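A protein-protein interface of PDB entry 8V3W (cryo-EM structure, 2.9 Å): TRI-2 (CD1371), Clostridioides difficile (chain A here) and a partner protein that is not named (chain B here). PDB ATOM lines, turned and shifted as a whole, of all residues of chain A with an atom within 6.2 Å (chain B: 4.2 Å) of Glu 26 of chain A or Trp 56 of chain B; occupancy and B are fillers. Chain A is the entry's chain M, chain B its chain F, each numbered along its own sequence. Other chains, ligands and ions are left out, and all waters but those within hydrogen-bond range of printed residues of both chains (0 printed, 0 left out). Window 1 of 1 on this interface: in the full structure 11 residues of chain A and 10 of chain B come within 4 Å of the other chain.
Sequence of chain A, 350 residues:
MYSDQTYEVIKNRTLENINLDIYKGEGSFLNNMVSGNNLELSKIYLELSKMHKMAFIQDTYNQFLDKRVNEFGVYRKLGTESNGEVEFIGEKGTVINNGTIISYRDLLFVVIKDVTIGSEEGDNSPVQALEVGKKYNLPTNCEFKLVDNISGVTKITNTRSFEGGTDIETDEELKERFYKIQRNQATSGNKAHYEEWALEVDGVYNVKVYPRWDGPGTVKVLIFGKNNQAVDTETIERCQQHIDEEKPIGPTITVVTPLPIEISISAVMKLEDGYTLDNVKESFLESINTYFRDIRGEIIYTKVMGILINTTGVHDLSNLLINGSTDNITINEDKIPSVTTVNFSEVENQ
The indole nitrogen of Trp 56 of chain B is in hydrogen-bond range of the backbone carbonyl oxygen of Glu 26 of chain A, 3.2 Å away. The side-chain carboxylate (OE1) of Glu 26 of chain A lies within hydrogen-bond range of the side-chain hydroxyl (OG) of Ser 72 of chain B (2.5 Å). OH of Tyr 71 of chain B sits at hydrogen-bond distance from OD1 of Asn 32 of chain A (3.1 Å).
The backbone carbonyl oxygen (O) of Ser 28 of chain A sits close to the side-chain amide nitrogen (ND2) of Asn 32 of chain A (3.5 Å).
OD1 of Asn 107 of chain B touches OH of Tyr 23 of chain A, at 3.8 Å. Glu 74 of chain B touches Glu 26 of chain A (OE2 to OE1, 3.8 Å). OE1 of Glu 26 of chain A touches CB of Tyr 75 of chain B, at 3.7 Å. O of Gly 27 of chain A touches CD1 of Trp 56 of chain B, at 3.8 Å. CA of Gly 27 of chain A touches OH of Tyr 75 of chain B, 3.5 Å away.
Glu 26 of chain A touches just these residues of chain B: Trp 56 (3.2 Å), Ser 72 (2.5 Å), Glu 74 (3.8 Å) and Tyr 75 (3.7 Å). Of chain A, only Glu 26 and Gly 27 come within 4 Å of Trp 56 of chain B. Printed residues of chain A within 4 Å of Glu 74 of chain B: Glu 26. Printed residues of chain A within 4 Å of Ser 72 of chain B: Glu 26. Of the printed residues of chain B, Tyr 23 of chain A touches Asn 107. Cys 60 of chain B touches none of the printed residues of chain A. The nearest residue of chain B that does not touch Glu 26 of chain A is Tyr 71 of chain B (4.03 Å). The nearest residue of chain A that does not touch Trp 56 of chain B is Tyr 23 of chain A (4.4 Å). The nearest printed residue of chain A that does not touch Tyr 71 of chain B is Glu 26 of chain A (4.03 Å).
Of the 9 printed residues of chain A, 4 touch a printed residue of chain B. Hydrophobic or aromatic side chains of chain B within 4 Å of the printed part of chain A: Trp 56, Tyr 71 and Tyr 75. Among the printed residues, no Asp or Glu carboxylate lies within 4 Å of a Lys or Arg side-chain nitrogen of the other chain.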
ATOM      1  N   LYS A  11      41.407  34.294  -0.170  1.00  0.00           N
ATOM      2  CA  LYS A  11      40.345  33.303  -0.035  1.00  0.00           C
ATOM      3  C   LYS A  11      40.912  31.901   0.122  1.00  0.00           C
ATOM      4  O   LYS A  11      40.441  31.122   0.959  1.00  0.00           O
ATOM      5  CB  LYS A  11      39.426  33.371  -1.249  1.00  0.00           C
ATOM      6  CG  LYS A  11      38.064  32.756  -1.055  1.00  0.00           C
ATOM      7  CD  LYS A  11      37.447  32.464  -2.400  1.00  0.00           C
ATOM      8  CE  LYS A  11      35.952  32.598  -2.365  1.00  0.00           C
ATOM      9  NZ  LYS A  11      35.376  32.664  -3.735  1.00  0.00           N
ATOM     10  N   TYR A  23      32.655  20.011   2.268  1.00  0.00           N
ATOM     11  CA  TYR A  23      33.300  20.289   0.993  1.00  0.00           C
ATOM     12  C   TYR A  23      33.457  21.790   0.797  1.00  0.00           C
ATOM     13  O   TYR A  23      32.497  22.550   0.952  1.00  0.00           O
ATOM     14  CB  TYR A  23      32.478  19.675  -0.142  1.00  0.00           C
ATOM     15  CG  TYR A  23      32.706  20.265  -1.517  1.00  0.00           C
ATOM     16  CD1 TYR A  23      33.749  19.825  -2.315  1.00  0.00           C
ATOM     17  CD2 TYR A  23      31.854  21.231  -2.031  1.00  0.00           C
ATOM     18  CE1 TYR A  23      33.953  20.343  -3.573  1.00  0.00           C
ATOM     19  CE2 TYR A  23      32.051  21.756  -3.289  1.00  0.00           C
ATOM     20  CZ  TYR A  23      33.103  21.309  -4.055  1.00  0.00           C
ATOM     21  OH  TYR A  23      33.306  21.828  -5.310  1.00  0.00           O
ATOM     22  N   LYS A  24      34.670  22.216   0.460  1.00  0.00           N
ATOM     23  CA  LYS A  24      34.995  23.623   0.264  1.00  0.00           C
ATOM     24  C   LYS A  24      35.284  23.841  -1.213  1.00  0.00           C
ATOM     25  O   LYS A  24      36.348  23.455  -1.707  1.00  0.00           O
ATOM     26  CB  LYS A  24      36.192  24.034   1.118  1.00  0.00           C
ATOM     27  CG  LYS A  24      36.091  23.624   2.572  1.00  0.00           C
ATOM     28  CD  LYS A  24      37.111  24.361   3.413  1.00  0.00           C
ATOM     29  CE  LYS A  24      37.421  23.616   4.693  1.00  0.00           C
ATOM     30  NZ  LYS A  24      38.695  22.861   4.582  1.00  0.00           N
ATOM     31  N   GLY A  25      34.346  24.467  -1.913  1.00  0.00           N
ATOM     32  CA  GLY A  25      34.504  24.720  -3.332  1.00  0.00           C
ATOM     33  C   GLY A  25      33.506  25.764  -3.766  1.00  0.00           C
ATOM     34  O   GLY A  25      32.640  26.183  -2.996  1.00  0.00           O
ATOM     35  N   GLU A  26      33.640  26.189  -5.020  1.00  0.00           N
ATOM     36  CA  GLU A  26      32.754  27.219  -5.543  1.00  0.00           C
ATOM     37  C   GLU A  26      31.311  26.741  -5.495  1.00  0.00           C
ATOM     38  O   GLU A  26      30.995  25.637  -5.946  1.00  0.00           O
ATOM     39  CB  GLU A  26      33.144  27.581  -6.975  1.00  0.00           C
ATOM     40  CG  GLU A  26      32.509  28.866  -7.475  1.00  0.00           C
ATOM     41  CD  GLU A  26      33.450  29.705  -8.310  1.00  0.00           C
ATOM     42  OE1 GLU A  26      33.636  29.383  -9.500  1.00  0.00           O
ATOM     43  OE2 GLU A  26      34.004  30.688  -7.780  1.00  0.00           O
ATOM     44  N   GLY A  27      30.439  27.573  -4.941  1.00  0.00           N
ATOM     45  CA  GLY A  27      29.041  27.232  -4.806  1.00  0.00           C
ATOM     46  C   GLY A  27      28.649  26.554  -3.513  1.00  0.00           C
ATOM     47  O   GLY A  27      27.488  26.160  -3.372  1.00  0.00           O
ATOM     48  N   SER A  28      29.570  26.406  -2.567  1.00  0.00           N
ATOM     49  CA  SER A  28      29.271  25.780  -1.290  1.00  0.00           C
ATOM     50  C   SER A  28      28.839  26.825  -0.266  1.00  0.00           C
ATOM     51  O   SER A  28      29.042  28.027  -0.442  1.00  0.00           O
ATOM     52  CB  SER A  28      30.485  25.014  -0.772  1.00  0.00           C
ATOM     53  OG  SER A  28      31.163  24.376  -1.832  1.00  0.00           O
ATOM     54  N   ASN A  31      32.049  28.381   1.452  1.00  0.00           N
ATOM     55  CA  ASN A  31      32.677  29.275   0.490  1.00  0.00           C
ATOM     56  C   ASN A  31      31.868  30.554   0.318  1.00  0.00           C
ATOM     57  O   ASN A  31      32.432  31.652   0.268  1.00  0.00           O
ATOM     58  CB  ASN A  31      32.850  28.542  -0.841  1.00  0.00           C
ATOM     59  CG  ASN A  31      33.732  29.284  -1.817  1.00  0.00           C
ATOM     60  OD1 ASN A  31      33.712  30.506  -1.889  1.00  0.00           O
ATOM     61  ND2 ASN A  31      34.524  28.540  -2.572  1.00  0.00           N
ATOM     62  N   ASN A  32      30.543  30.435   0.233  1.00  0.00           N
ATOM     63  CA  ASN A  32      29.705  31.620   0.082  1.00  0.00           C
ATOM     64  C   ASN A  32      29.810  32.528   1.300  1.00  0.00           C
ATOM     65  O   ASN A  32      29.852  33.755   1.166  1.00  0.00           O
ATOM     66  CB  ASN A  32      28.254  31.208  -0.156  1.00  0.00           C
ATOM     67  CG  ASN A  32      27.990  30.807  -1.588  1.00  0.00           C
ATOM     68  OD1 ASN A  32      28.849  30.952  -2.455  1.00  0.00           O
ATOM     69  ND2 ASN A  32      26.801  30.284  -1.843  1.00  0.00           N
ATOM     70  N   ALA B  52      23.489  15.870  -0.523  1.00  0.00           N
ATOM     71  CA  ALA B  52      24.274  17.095  -0.606  1.00  0.00           C
ATOM     72  C   ALA B  52      24.368  17.601  -2.041  1.00  0.00           C
ATOM     73  O   ALA B  52      24.345  18.818  -2.285  1.00  0.00           O
ATOM     74  CB  ALA B  52      25.667  16.854  -0.033  1.00  0.00           C
ATOM     75  N   LEU B  53      24.482  16.679  -2.997  1.00  0.00           N
ATOM     76  CA  LEU B  53      24.528  17.073  -4.397  1.00  0.00           C
ATOM     77  C   LEU B  53      23.239  17.759  -4.818  1.00  0.00           C
ATOM     78  O   LEU B  53      23.263  18.636  -5.685  1.00  0.00           O
ATOM     79  CB  LEU B  53      24.803  15.854  -5.274  1.00  0.00           C
ATOM     80  CG  LEU B  53      26.240  15.343  -5.227  1.00  0.00           C
ATOM     81  CD1 LEU B  53      26.410  14.130  -6.113  1.00  0.00           C
ATOM     82  CD2 LEU B  53      27.209  16.431  -5.629  1.00  0.00           C
ATOM     83  N   LYS B  54      22.111  17.385  -4.214  1.00  0.00           N
ATOM     84  CA  LYS B  54      20.864  18.087  -4.501  1.00  0.00           C
ATOM     85  C   LYS B  54      20.968  19.558  -4.127  1.00  0.00           C
ATOM     86  O   LYS B  54      20.563  20.438  -4.896  1.00  0.00           O
ATOM     87  CB  LYS B  54      19.700  17.432  -3.761  1.00  0.00           C
ATOM     88  CG  LYS B  54      19.256  16.107  -4.328  1.00  0.00           C
ATOM     89  CD  LYS B  54      17.976  15.646  -3.659  1.00  0.00           C
ATOM     90  CE  LYS B  54      17.634  14.226  -4.050  1.00  0.00           C
ATOM     91  NZ  LYS B  54      16.305  13.818  -3.525  1.00  0.00           N
ATOM     92  N   VAL B  55      21.518  19.843  -2.945  1.00  0.00           N
ATOM     93  CA  VAL B  55      21.691  21.226  -2.515  1.00  0.00           C
ATOM     94  C   VAL B  55      22.619  21.964  -3.464  1.00  0.00           C
ATOM     95  O   VAL B  55      22.343  23.102  -3.874  1.00  0.00           O
ATOM     96  CB  VAL B  55      22.219  21.270  -1.070  1.00  0.00           C
ATOM     97  CG1 VAL B  55      22.482  22.698  -0.652  1.00  0.00           C
ATOM     98  CG2 VAL B  55      21.242  20.604  -0.122  1.00  0.00           C
ATOM     99  N   TRP B  56      23.736  21.331  -3.830  1.00  0.00           N
ATOM    100  CA  TRP B  56      24.684  22.003  -4.714  1.00  0.00           C
ATOM    101  C   TRP B  56      24.057  22.319  -6.067  1.00  0.00           C
ATOM    102  O   TRP B  56      24.242  23.416  -6.602  1.00  0.00           O
ATOM    103  CB  TRP B  56      25.946  21.167  -4.898  1.00  0.00           C
ATOM    104  CG  TRP B  56      27.033  21.948  -5.562  1.00  0.00           C
ATOM    105  CD1 TRP B  56      27.986  22.700  -4.952  1.00  0.00           C
ATOM    106  CD2 TRP B  56      27.263  22.075  -6.971  1.00  0.00           C
ATOM    107  NE1 TRP B  56      28.802  23.283  -5.888  1.00  0.00           N
ATOM    108  CE2 TRP B  56      28.378  22.914  -7.136  1.00  0.00           C
ATOM    109  CE3 TRP B  56      26.636  21.558  -8.108  1.00  0.00           C
ATOM    110  CZ2 TRP B  56      28.880  23.248  -8.389  1.00  0.00           C
ATOM    111  CZ3 TRP B  56      27.135  21.891  -9.349  1.00  0.00           C
ATOM    112  CH2 TRP B  56      28.246  22.727  -9.481  1.00  0.00           C
ATOM    113  N   ILE B  57      23.311  21.371  -6.636  1.00  0.00           N
ATOM    114  CA  ILE B  57      22.686  21.593  -7.935  1.00  0.00           C
ATOM    115  C   ILE B  57      21.633  22.686  -7.848  1.00  0.00           C
ATOM    116  O   ILE B  57      21.534  23.542  -8.735  1.00  0.00           O
ATOM    117  CB  ILE B  57      22.092  20.278  -8.469  1.00  0.00           C
ATOM    118  CG1 ILE B  57      23.208  19.324  -8.880  1.00  0.00           C
ATOM    119  CG2 ILE B  57      21.162  20.552  -9.634  1.00  0.00           C
ATOM    120  CD1 ILE B  57      22.742  17.915  -9.106  1.00  0.00           C
ATOM    121  N   TYR B  58      20.817  22.667  -6.794  1.00  0.00           N
ATOM    122  CA  TYR B  58      19.798  23.696  -6.623  1.00  0.00           C
ATOM    123  C   TYR B  58      20.432  25.079  -6.574  1.00  0.00           C
ATOM    124  O   TYR B  58      20.005  26.005  -7.282  1.00  0.00           O
ATOM    125  CB  TYR B  58      19.003  23.406  -5.350  1.00  0.00           C
ATOM    126  CG  TYR B  58      17.928  24.404  -5.010  1.00  0.00           C
ATOM    127  CD1 TYR B  58      18.203  25.509  -4.222  1.00  0.00           C
ATOM    128  CD2 TYR B  58      16.630  24.225  -5.451  1.00  0.00           C
ATOM    129  CE1 TYR B  58      17.222  26.413  -3.901  1.00  0.00           C
ATOM    130  CE2 TYR B  58      15.644  25.122  -5.135  1.00  0.00           C
ATOM    131  CZ  TYR B  58      15.942  26.214  -4.360  1.00  0.00           C
ATOM    132  OH  TYR B  58      14.954  27.113  -4.044  1.00  0.00           O
ATOM    133  N   LYS B  59      21.488  25.223  -5.774  1.00  0.00           N
ATOM    134  CA  LYS B  59      22.156  26.514  -5.667  1.00  0.00           C
ATOM    135  C   LYS B  59      22.794  26.922  -6.989  1.00  0.00           C
ATOM    136  O   LYS B  59      22.743  28.096  -7.365  1.00  0.00           O
ATOM    137  CB  LYS B  59      23.192  26.475  -4.548  1.00  0.00           C
ATOM    138  CG  LYS B  59      22.600  26.718  -3.174  1.00  0.00           C
ATOM    139  CD  LYS B  59      23.646  27.234  -2.219  1.00  0.00           C
ATOM    140  CE  LYS B  59      23.858  26.279  -1.070  1.00  0.00           C
ATOM    141  NZ  LYS B  59      23.157  26.748   0.146  1.00  0.00           N
ATOM    142  N   CYS B  60      23.399  25.976  -7.711  1.00  0.00           N
ATOM    143  CA  CYS B  60      24.037  26.326  -8.977  1.00  0.00           C
ATOM    144  C   CYS B  60      23.018  26.790 -10.007  1.00  0.00           C
ATOM    145  O   CYS B  60      23.248  27.773 -10.719  1.00  0.00           O
ATOM    146  CB  CYS B  60      24.835  25.147  -9.524  1.00  0.00           C
ATOM    147  SG  CYS B  60      25.634  25.482 -11.107  1.00  0.00           S
ATOM    148  N   TYR B  71      32.015  35.409  -7.751  1.00  0.00           N
ATOM    149  CA  TYR B  71      32.114  34.171  -8.504  1.00  0.00           C
ATOM    150  C   TYR B  71      33.009  34.340  -9.725  1.00  0.00           C
ATOM    151  O   TYR B  71      33.255  35.449 -10.200  1.00  0.00           O
ATOM    152  CB  TYR B  71      30.731  33.693  -8.942  1.00  0.00           C
ATOM    153  CG  TYR B  71      29.803  33.365  -7.800  1.00  0.00           C
ATOM    154  CD1 TYR B  71      30.185  32.490  -6.800  1.00  0.00           C
ATOM    155  CD2 TYR B  71      28.539  33.926  -7.730  1.00  0.00           C
ATOM    156  CE1 TYR B  71      29.337  32.187  -5.761  1.00  0.00           C
ATOM    157  CE2 TYR B  71      27.687  33.630  -6.696  1.00  0.00           C
ATOM    158  CZ  TYR B  71      28.090  32.762  -5.715  1.00  0.00           C
ATOM    159  OH  TYR B  71      27.238  32.465  -4.681  1.00  0.00           O
ATOM    160  N   SER B  72      33.485  33.213 -10.240  1.00  0.00           N
ATOM    161  CA  SER B  72      34.299  33.199 -11.445  1.00  0.00           C
ATOM    162  C   SER B  72      33.390  33.269 -12.671  1.00  0.00           C
ATOM    163  O   SER B  72      32.178  33.467 -12.565  1.00  0.00           O
ATOM    164  CB  SER B  72      35.195  31.967 -11.457  1.00  0.00           C
ATOM    165  OG  SER B  72      34.419  30.785 -11.478  1.00  0.00           O
ATOM    166  N   GLU B  74      32.745  30.825 -14.740  1.00  0.00           N
ATOM    167  CA  GLU B  74      32.174  29.531 -15.080  1.00  0.00           C
ATOM    168  C   GLU B  74      30.999  29.135 -14.198  1.00  0.00           C
ATOM    169  O   GLU B  74      30.248  28.229 -14.571  1.00  0.00           O
ATOM    170  CB  GLU B  74      33.247  28.442 -14.994  1.00  0.00           C
ATOM    171  CG  GLU B  74      34.111  28.555 -13.757  1.00  0.00           C
ATOM    172  CD  GLU B  74      34.762  27.244 -13.374  1.00  0.00           C
ATOM    173  OE1 GLU B  74      34.976  26.401 -14.268  1.00  0.00           O
ATOM    174  OE2 GLU B  74      35.050  27.056 -12.173  1.00  0.00           O
ATOM    175  N   TYR B  75      30.822  29.780 -13.051  1.00  0.00           N
ATOM    176  CA  TYR B  75      29.760  29.418 -12.124  1.00  0.00           C
ATOM    177  C   TYR B  75      28.468  30.137 -12.477  1.00  0.00           C
ATOM    178  O   TYR B  75      28.469  31.330 -12.782  1.00  0.00           O
ATOM    179  CB  TYR B  75      30.163  29.744 -10.685  1.00  0.00           C
ATOM    180  CG  TYR B  75      29.156  29.285  -9.657  1.00  0.00           C
ATOM    181  CD1 TYR B  75      29.111  27.966  -9.237  1.00  0.00           C
ATOM    182  CD2 TYR B  75      28.244  30.172  -9.115  1.00  0.00           C
ATOM    183  CE1 TYR B  75      28.191  27.549  -8.304  1.00  0.00           C
ATOM    184  CE2 TYR B  75      27.320  29.764  -8.186  1.00  0.00           C
ATOM    185  CZ  TYR B  75      27.297  28.452  -7.784  1.00  0.00           C
ATOM    186  OH  TYR B  75      26.372  28.046  -6.854  1.00  0.00           O
ATOM    187  N   ILE B 106      30.642  21.339 -14.322  1.00  0.00           N
ATOM    188  CA  ILE B 106      31.927  21.741 -13.750  1.00  0.00           C
ATOM    189  C   ILE B 106      32.256  20.994 -12.463  1.00  0.00           C
ATOM    190  O   ILE B 106      33.431  20.903 -12.094  1.00  0.00           O
ATOM    191  CB  ILE B 106      31.985  23.259 -13.500  1.00  0.00           C
ATOM    192  CG1 ILE B 106      30.920  23.686 -12.493  1.00  0.00           C
ATOM    193  CG2 ILE B 106      31.838  24.019 -14.800  1.00  0.00           C
ATOM    194  CD1 ILE B 106      31.204  25.017 -11.854  1.00  0.00           C
ATOM    195  N   ASN B 107      31.260  20.465 -11.766  1.00  0.00           N
ATOM    196  CA  ASN B 107      31.517  19.729 -10.532  1.00  0.00           C
ATOM    197  C   ASN B 107      32.180  18.392 -10.848  1.00  0.00           C
ATOM    198  O   ASN B 107      31.665  17.631 -11.672  1.00  0.00           O
ATOM    199  CB  ASN B 107      30.212  19.505  -9.775  1.00  0.00           C
ATOM    200  CG  ASN B 107      30.421  19.331  -8.289  1.00  0.00           C
ATOM    201  OD1 ASN B 107      31.484  19.631  -7.761  1.00  0.00           O
ATOM    202  ND2 ASN B 107      29.398  18.842  -7.605  1.00  0.00           N
